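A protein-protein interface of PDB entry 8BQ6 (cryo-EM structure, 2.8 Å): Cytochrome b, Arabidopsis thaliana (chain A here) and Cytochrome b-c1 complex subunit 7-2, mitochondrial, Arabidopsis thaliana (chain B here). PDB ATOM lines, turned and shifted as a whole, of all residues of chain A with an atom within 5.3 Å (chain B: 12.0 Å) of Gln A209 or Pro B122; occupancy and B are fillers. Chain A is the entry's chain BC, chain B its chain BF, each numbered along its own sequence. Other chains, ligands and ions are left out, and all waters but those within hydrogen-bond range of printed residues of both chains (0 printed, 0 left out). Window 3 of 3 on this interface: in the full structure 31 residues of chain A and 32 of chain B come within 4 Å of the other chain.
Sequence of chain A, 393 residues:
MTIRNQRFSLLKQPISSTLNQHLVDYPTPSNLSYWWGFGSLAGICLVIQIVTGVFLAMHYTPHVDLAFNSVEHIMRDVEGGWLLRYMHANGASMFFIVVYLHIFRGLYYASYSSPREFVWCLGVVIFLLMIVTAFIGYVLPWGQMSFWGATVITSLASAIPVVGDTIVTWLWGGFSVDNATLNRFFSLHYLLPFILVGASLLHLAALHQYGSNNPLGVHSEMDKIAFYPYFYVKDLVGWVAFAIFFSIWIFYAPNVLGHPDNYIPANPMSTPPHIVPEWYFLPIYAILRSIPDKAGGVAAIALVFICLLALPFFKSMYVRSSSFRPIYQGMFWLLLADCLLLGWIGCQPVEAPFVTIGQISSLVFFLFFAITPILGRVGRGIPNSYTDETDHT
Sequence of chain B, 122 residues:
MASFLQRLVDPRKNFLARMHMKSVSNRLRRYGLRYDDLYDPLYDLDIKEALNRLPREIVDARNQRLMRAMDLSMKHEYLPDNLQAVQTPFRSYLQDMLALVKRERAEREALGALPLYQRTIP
O of Pro A115 sits at hydrogen-bond distance from NH2 of Arg B119 (3.0 Å). The side-chain carboxylate (OE2) of Glu A117 lies within salt-bridge range of the guanidinium group (NH2) of Arg B119. OG1 of Thr B120 is in hydrogen-bond range of OH of Tyr A210 (3.5 Å).
OD1 of Asp B40 sits at hydrogen-bond distance from N of Leu B42 (2.6 Å).
Among the printed residues, pairs that only touch across the chains: Pro A115 with Leu B42 (3.5 Å) and Gln A209 with Pro B122 (3.8 Å).
Of the printed residues of chain B, Pro A115 touches Leu B42 and Arg B119. Of chain B, only Arg B119 (2.7 Å) comes within 4 Å of Glu A117. No residue of chain B comes within 4 Å of Ala A205. No residue of chain B comes within 4 Å of Leu A207. Gln A209 touches one residue of chain B. No residue of chain B comes within 4 Å of Gly A211. Gln B118 touches none of the printed residues of chain A. Of the printed residues of chain A, Arg B119 touches Pro A115 (3.0 Å) and Glu A117 (2.7 Å). Of the printed residues of chain A, Thr B120 touches Tyr A210 (3.5 Å).
Hydrophobic or aromatic side chains of chain B that line the printed part of chain A: Leu B42 and Pro B122. Of the 11 printed residues of chain A, 4 touch a printed residue of chain B. Printed residues of chain A that touch a printed residue of chain B: Pro A115, Glu A117, Gln A209 and Tyr A210. Hydrophobic or aromatic side chains of chain A within 4 Å of the printed part of chain B: Pro A115 and Tyr A210. Among the printed residues, 5 pairs touch across the chains.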
ATOM      1  N   TYR A  26      39.912  -4.658  22.986  1.00  0.00           N
ATOM      2  CA  TYR A  26      38.728  -4.327  22.208  1.00  0.00           C
ATOM      3  C   TYR A  26      37.611  -5.326  22.491  1.00  0.00           C
ATOM      4  O   TYR A  26      37.841  -6.541  22.428  1.00  0.00           O
ATOM      5  CB  TYR A  26      39.032  -4.295  20.713  1.00  0.00           C
ATOM      6  CG  TYR A  26      37.927  -3.620  19.942  1.00  0.00           C
ATOM      7  CD1 TYR A  26      37.775  -2.245  19.981  1.00  0.00           C
ATOM      8  CD2 TYR A  26      37.010  -4.359  19.213  1.00  0.00           C
ATOM      9  CE1 TYR A  26      36.760  -1.625  19.299  1.00  0.00           C
ATOM     10  CE2 TYR A  26      35.993  -3.748  18.525  1.00  0.00           C
ATOM     11  CZ  TYR A  26      35.871  -2.381  18.573  1.00  0.00           C
ATOM     12  OH  TYR A  26      34.854  -1.764  17.893  1.00  0.00           O
ATOM     13  N   PRO A 115      24.945  -1.717  10.627  1.00  0.00           N
ATOM     14  CA  PRO A 115      25.622  -0.441  10.329  1.00  0.00           C
ATOM     15  C   PRO A 115      27.032  -0.573   9.735  1.00  0.00           C
ATOM     16  O   PRO A 115      27.817   0.319   9.929  1.00  0.00           O
ATOM     17  CB  PRO A 115      25.692   0.095  11.759  1.00  0.00           C
ATOM     18  CG  PRO A 115      26.055  -1.118  12.590  1.00  0.00           C
ATOM     19  CD  PRO A 115      25.416  -2.293  11.884  1.00  0.00           C
ATOM     20  N   GLU A 117      28.091  -0.944   6.306  1.00  0.00           N
ATOM     21  CA  GLU A 117      28.095  -0.890   4.825  1.00  0.00           C
ATOM     22  C   GLU A 117      29.470  -0.420   4.347  1.00  0.00           C
ATOM     23  O   GLU A 117      29.935  -0.952   3.335  1.00  0.00           O
ATOM     24  CB  GLU A 117      26.964   0.006   4.324  1.00  0.00           C
ATOM     25  CG  GLU A 117      25.615  -0.334   4.918  1.00  0.00           C
ATOM     26  CD  GLU A 117      25.135   0.697   5.919  1.00  0.00           C
ATOM     27  OE1 GLU A 117      24.175   1.424   5.606  1.00  0.00           O
ATOM     28  OE2 GLU A 117      25.733   0.776   7.002  1.00  0.00           O
ATOM     29  N   PHE A 118      30.097   0.522   5.060  1.00  0.00           N
ATOM     30  CA  PHE A 118      31.431   0.995   4.705  1.00  0.00           C
ATOM     31  C   PHE A 118      32.464  -0.112   4.850  1.00  0.00           C
ATOM     32  O   PHE A 118      33.455  -0.147   4.110  1.00  0.00           O
ATOM     33  CB  PHE A 118      31.803   2.193   5.577  1.00  0.00           C
ATOM     34  CG  PHE A 118      32.968   2.989   5.061  1.00  0.00           C
ATOM     35  CD1 PHE A 118      33.067   3.303   3.718  1.00  0.00           C
ATOM     36  CD2 PHE A 118      33.949   3.447   5.924  1.00  0.00           C
ATOM     37  CE1 PHE A 118      34.131   4.045   3.241  1.00  0.00           C
ATOM     38  CE2 PHE A 118      35.015   4.194   5.453  1.00  0.00           C
ATOM     39  CZ  PHE A 118      35.104   4.492   4.110  1.00  0.00           C
ATOM     40  N   ALA A 205      39.749  -0.427  10.841  1.00  0.00           N
ATOM     41  CA  ALA A 205      39.298   0.736  11.596  1.00  0.00           C
ATOM     42  C   ALA A 205      37.804   0.973  11.409  1.00  0.00           C
ATOM     43  O   ALA A 205      37.088   1.285  12.366  1.00  0.00           O
ATOM     44  CB  ALA A 205      40.096   1.969  11.175  1.00  0.00           C
ATOM     45  N   ALA A 206      37.316   0.838  10.173  1.00  0.00           N
ATOM     46  CA  ALA A 206      35.898   1.066   9.911  1.00  0.00           C
ATOM     47  C   ALA A 206      35.031   0.039  10.627  1.00  0.00           C
ATOM     48  O   ALA A 206      33.907   0.346  11.042  1.00  0.00           O
ATOM     49  CB  ALA A 206      35.627   1.039   8.409  1.00  0.00           C
ATOM     50  N   LEU A 207      35.525  -1.191  10.767  1.00  0.00           N
ATOM     51  CA  LEU A 207      34.750  -2.205  11.470  1.00  0.00           C
ATOM     52  C   LEU A 207      34.698  -1.918  12.963  1.00  0.00           C
ATOM     53  O   LEU A 207      33.652  -2.089  13.600  1.00  0.00           O
ATOM     54  CB  LEU A 207      35.335  -3.590  11.214  1.00  0.00           C
ATOM     55  CG  LEU A 207      34.738  -4.690  12.087  1.00  0.00           C
ATOM     56  CD1 LEU A 207      33.352  -5.063  11.607  1.00  0.00           C
ATOM     57  CD2 LEU A 207      35.639  -5.886  12.092  1.00  0.00           C
ATOM     58  N   HIS A 208      35.810  -1.455  13.534  1.00  0.00           N
ATOM     59  CA  HIS A 208      35.872  -1.223  14.968  1.00  0.00           C
ATOM     60  C   HIS A 208      34.997  -0.064  15.419  1.00  0.00           C
ATOM     61  O   HIS A 208      34.819   0.120  16.627  1.00  0.00           O
ATOM     62  CB  HIS A 208      37.315  -0.986  15.401  1.00  0.00           C
ATOM     63  CG  HIS A 208      38.094  -2.248  15.590  1.00  0.00           C
ATOM     64  ND1 HIS A 208      39.299  -2.290  16.255  1.00  0.00           N
ATOM     65  CD2 HIS A 208      37.841  -3.516  15.190  1.00  0.00           C
ATOM     66  CE1 HIS A 208      39.752  -3.530  16.264  1.00  0.00           C
ATOM     67  NE2 HIS A 208      38.886  -4.294  15.624  1.00  0.00           N
ATOM     68  N   GLN A 209      34.458   0.725  14.489  1.00  0.00           N
ATOM     69  CA  GLN A 209      33.512   1.767  14.868  1.00  0.00           C
ATOM     70  C   GLN A 209      32.227   1.167  15.429  1.00  0.00           C
ATOM     71  O   GLN A 209      31.529   1.803  16.227  1.00  0.00           O
ATOM     72  CB  GLN A 209      33.228   2.655  13.659  1.00  0.00           C
ATOM     73  CG  GLN A 209      32.019   3.551  13.794  1.00  0.00           C
ATOM     74  CD  GLN A 209      31.574   4.099  12.462  1.00  0.00           C
ATOM     75  OE1 GLN A 209      31.992   3.617  11.411  1.00  0.00           O
ATOM     76  NE2 GLN A 209      30.721   5.114  12.494  1.00  0.00           N
ATOM     77  N   TYR A 210      31.928  -0.085  15.103  1.00  0.00           N
ATOM     78  CA  TYR A 210      30.652  -0.702  15.553  1.00  0.00           C
ATOM     79  C   TYR A 210      30.894  -2.081  16.159  1.00  0.00           C
ATOM     80  O   TYR A 210      29.973  -2.607  16.803  1.00  0.00           O
ATOM     81  CB  TYR A 210      29.688  -0.832  14.373  1.00  0.00           C
ATOM     82  CG  TYR A 210      29.055   0.462  13.934  1.00  0.00           C
ATOM     83  CD1 TYR A 210      29.354   1.016  12.703  1.00  0.00           C
ATOM     84  CD2 TYR A 210      28.164   1.136  14.751  1.00  0.00           C
ATOM     85  CE1 TYR A 210      28.776   2.202  12.288  1.00  0.00           C
ATOM     86  CE2 TYR A 210      27.579   2.326  14.353  1.00  0.00           C
ATOM     87  CZ  TYR A 210      27.887   2.862  13.117  1.00  0.00           C
ATOM     88  OH  TYR A 210      27.320   4.033  12.708  1.00  0.00           O
ATOM     89  N   GLY A 211      32.081  -2.654  15.959  1.00  0.00           N
ATOM     90  CA  GLY A 211      32.318  -3.999  16.425  1.00  0.00           C
ATOM     91  C   GLY A 211      31.831  -5.020  15.420  1.00  0.00           C
ATOM     92  O   GLY A 211      31.055  -4.735  14.506  1.00  0.00           O
ATOM     93  N   ASP B  40      17.715  -4.953  15.679  1.00  0.00           N
ATOM     94  CA  ASP B  40      18.894  -4.340  16.285  1.00  0.00           C
ATOM     95  C   ASP B  40      18.732  -2.821  16.316  1.00  0.00           C
ATOM     96  O   ASP B  40      18.335  -2.233  15.306  1.00  0.00           O
ATOM     97  CB  ASP B  40      20.144  -4.725  15.486  1.00  0.00           C
ATOM     98  CG  ASP B  40      21.442  -4.269  16.142  1.00  0.00           C
ATOM     99  OD1 ASP B  40      21.409  -3.344  16.963  1.00  0.00           O
ATOM    100  OD2 ASP B  40      22.516  -4.831  15.832  1.00  0.00           O
ATOM    101  N   PRO B  41      19.006  -2.149  17.445  1.00  0.00           N
ATOM    102  CA  PRO B  41      19.062  -0.677  17.405  1.00  0.00           C
ATOM    103  C   PRO B  41      20.065  -0.140  16.399  1.00  0.00           C
ATOM    104  O   PRO B  41      19.808   0.891  15.772  1.00  0.00           O
ATOM    105  CB  PRO B  41      19.451  -0.284  18.840  1.00  0.00           C
ATOM    106  CG  PRO B  41      19.709  -1.556  19.580  1.00  0.00           C
ATOM    107  CD  PRO B  41      19.048  -2.664  18.824  1.00  0.00           C
ATOM    108  N   LEU B  42      21.208  -0.807  16.232  1.00  0.00           N
ATOM    109  CA  LEU B  42      22.216  -0.303  15.309  1.00  0.00           C
ATOM    110  C   LEU B  42      21.825  -0.507  13.856  1.00  0.00           C
ATOM    111  O   LEU B  42      22.457   0.080  12.972  1.00  0.00           O
ATOM    112  CB  LEU B  42      23.568  -0.961  15.581  1.00  0.00           C
ATOM    113  CG  LEU B  42      24.115  -0.787  16.996  1.00  0.00           C
ATOM    114  CD1 LEU B  42      25.485  -1.433  17.129  1.00  0.00           C
ATOM    115  CD2 LEU B  42      24.172   0.682  17.373  1.00  0.00           C
ATOM    116  N   TYR B  43      20.806  -1.321  13.584  1.00  0.00           N
ATOM    117  CA  TYR B  43      20.373  -1.494  12.205  1.00  0.00           C
ATOM    118  C   TYR B  43      19.789  -0.201  11.649  1.00  0.00           C
ATOM    119  O   TYR B  43      20.130   0.215  10.536  1.00  0.00           O
ATOM    120  CB  TYR B  43      19.370  -2.636  12.098  1.00  0.00           C
ATOM    121  CG  TYR B  43      19.159  -3.064  10.674  1.00  0.00           C
ATOM    122  CD1 TYR B  43      18.267  -2.397   9.852  1.00  0.00           C
ATOM    123  CD2 TYR B  43      19.896  -4.101  10.133  1.00  0.00           C
ATOM    124  CE1 TYR B  43      18.089  -2.775   8.542  1.00  0.00           C
ATOM    125  CE2 TYR B  43      19.729  -4.482   8.828  1.00  0.00           C
ATOM    126  CZ  TYR B  43      18.825  -3.819   8.036  1.00  0.00           C
ATOM    127  OH  TYR B  43      18.657  -4.206   6.729  1.00  0.00           O
ATOM    128  N   ASP B  44      18.911   0.452  12.402  1.00  0.00           N
ATOM    129  CA  ASP B  44      18.433   1.761  11.982  1.00  0.00           C
ATOM    130  C   ASP B  44      18.092   2.599  13.203  1.00  0.00           C
ATOM    131  O   ASP B  44      17.863   2.075  14.296  1.00  0.00           O
ATOM    132  CB  ASP B  44      17.235   1.658  11.020  1.00  0.00           C
ATOM    133  CG  ASP B  44      15.969   1.187  11.697  1.00  0.00           C
ATOM    134  OD1 ASP B  44      14.908   1.183  11.040  1.00  0.00           O
ATOM    135  OD2 ASP B  44      16.026   0.779  12.866  1.00  0.00           O
ATOM    136  N   LEU B  45      18.048   3.912  12.991  1.00  0.00           N
ATOM    137  CA  LEU B  45      17.750   4.846  14.100  1.00  0.00           C
ATOM    138  C   LEU B  45      16.263   4.772  14.482  1.00  0.00           C
ATOM    139  O   LEU B  45      15.933   5.287  15.561  1.00  0.00           O
ATOM    140  CB  LEU B  45      18.168   6.244  13.641  1.00  0.00           C
ATOM    141  CG  LEU B  45      19.441   6.801  14.280  1.00  0.00           C
ATOM    142  CD1 LEU B  45      19.240   7.055  15.765  1.00  0.00           C
ATOM    143  CD2 LEU B  45      20.623   5.874  14.055  1.00  0.00           C
ATOM    144  N   LYS B  48      16.066   2.109  17.310  1.00  0.00           N
ATOM    145  CA  LYS B  48      16.613   2.724  18.513  1.00  0.00           C
ATOM    146  C   LYS B  48      15.614   3.685  19.144  1.00  0.00           C
ATOM    147  O   LYS B  48      15.425   3.682  20.365  1.00  0.00           O
ATOM    148  CB  LYS B  48      17.922   3.437  18.181  1.00  0.00           C
ATOM    149  CG  LYS B  48      18.527   4.201  19.344  1.00  0.00           C
ATOM    150  CD  LYS B  48      19.983   4.546  19.089  1.00  0.00           C
ATOM    151  CE  LYS B  48      20.805   3.306  18.781  1.00  0.00           C
ATOM    152  NZ  LYS B  48      21.881   3.580  17.786  1.00  0.00           N
ATOM    153  N   GLN B 118      19.166  11.286  12.970  1.00  0.00           N
ATOM    154  CA  GLN B 118      19.773  10.877  11.684  1.00  0.00           C
ATOM    155  C   GLN B 118      20.877   9.862  11.990  1.00  0.00           C
ATOM    156  O   GLN B 118      21.350   9.827  13.144  1.00  0.00           O
ATOM    157  CB  GLN B 118      20.385  12.095  10.999  1.00  0.00           C
ATOM    158  CG  GLN B 118      19.532  12.702   9.899  1.00  0.00           C
ATOM    159  CD  GLN B 118      20.029  14.074   9.518  1.00  0.00           C
ATOM    160  OE1 GLN B 118      20.545  14.821  10.344  1.00  0.00           O
ATOM    161  NE2 GLN B 118      19.874  14.420   8.251  1.00  0.00           N
ATOM    162  N   ARG B 119      21.287   9.077  10.993  1.00  0.00           N
ATOM    163  CA  ARG B 119      22.395   8.103  11.197  1.00  0.00           C
ATOM    164  C   ARG B 119      23.741   8.807  10.975  1.00  0.00           C
ATOM    165  O   ARG B 119      23.847   9.603  10.023  1.00  0.00           O
ATOM    166  CB  ARG B 119      22.175   6.863  10.319  1.00  0.00           C
ATOM    167  CG  ARG B 119      23.226   5.770  10.446  1.00  0.00           C
ATOM    168  CD  ARG B 119      22.905   4.587   9.561  1.00  0.00           C
ATOM    169  NE  ARG B 119      23.888   3.519   9.655  1.00  0.00           N
ATOM    170  CZ  ARG B 119      24.999   3.478   8.934  1.00  0.00           C
ATOM    171  NH1 ARG B 119      25.254   4.444   8.071  1.00  0.00           N
ATOM    172  NH2 ARG B 119      25.847   2.476   9.075  1.00  0.00           N
ATOM    173  N   THR B 120      24.717   8.551  11.847  1.00  0.00           N
ATOM    174  CA  THR B 120      26.079   9.119  11.673  1.00  0.00           C
ATOM    175  C   THR B 120      26.725   8.533  10.417  1.00  0.00           C
ATOM    176  O   THR B 120      26.641   7.302  10.237  1.00  0.00           O
ATOM    177  CB  THR B 120      26.953   8.843  12.901  1.00  0.00           C
ATOM    178  OG1 THR B 120      26.946   7.443  13.183  1.00  0.00           O
ATOM    179  CG2 THR B 120      26.505   9.617  14.122  1.00  0.00           C
ATOM    180  N   ILE B 121      27.349   9.376   9.592  1.00  0.00           N
ATOM    181  CA  ILE B 121      27.981   8.901   8.323  1.00  0.00           C
ATOM    182  C   ILE B 121      29.183   8.024   8.679  1.00  0.00           C
ATOM    183  O   ILE B 121      30.164   8.568   9.221  1.00  0.00           O
ATOM    184  CB  ILE B 121      28.367  10.086   7.419  1.00  0.00           C
ATOM    185  CG1 ILE B 121      27.159  10.973   7.115  1.00  0.00           C
ATOM    186  CG2 ILE B 121      29.020   9.597   6.136  1.00  0.00           C
ATOM    187  CD1 ILE B 121      26.065  10.263   6.354  1.00  0.00           C
ATOM    188  N   PRO B 122      29.166   6.704   8.378  1.00  0.00           N
ATOM    189  CA  PRO B 122      30.245   5.808   8.794  1.00  0.00           C
ATOM    190  C   PRO B 122      31.566   6.192   8.121  1.00  0.00           C
ATOM    191  O   PRO B 122      32.501   6.405   8.864  1.00  0.00           O
ATOM    192  CB  PRO B 122      29.796   4.429   8.309  1.00  0.00           C
ATOM    193  CG  PRO B 122      28.847   4.730   7.172  1.00  0.00           C
ATOM    194  CD  PRO B 122      28.155   6.015   7.574  1.00  0.00           C
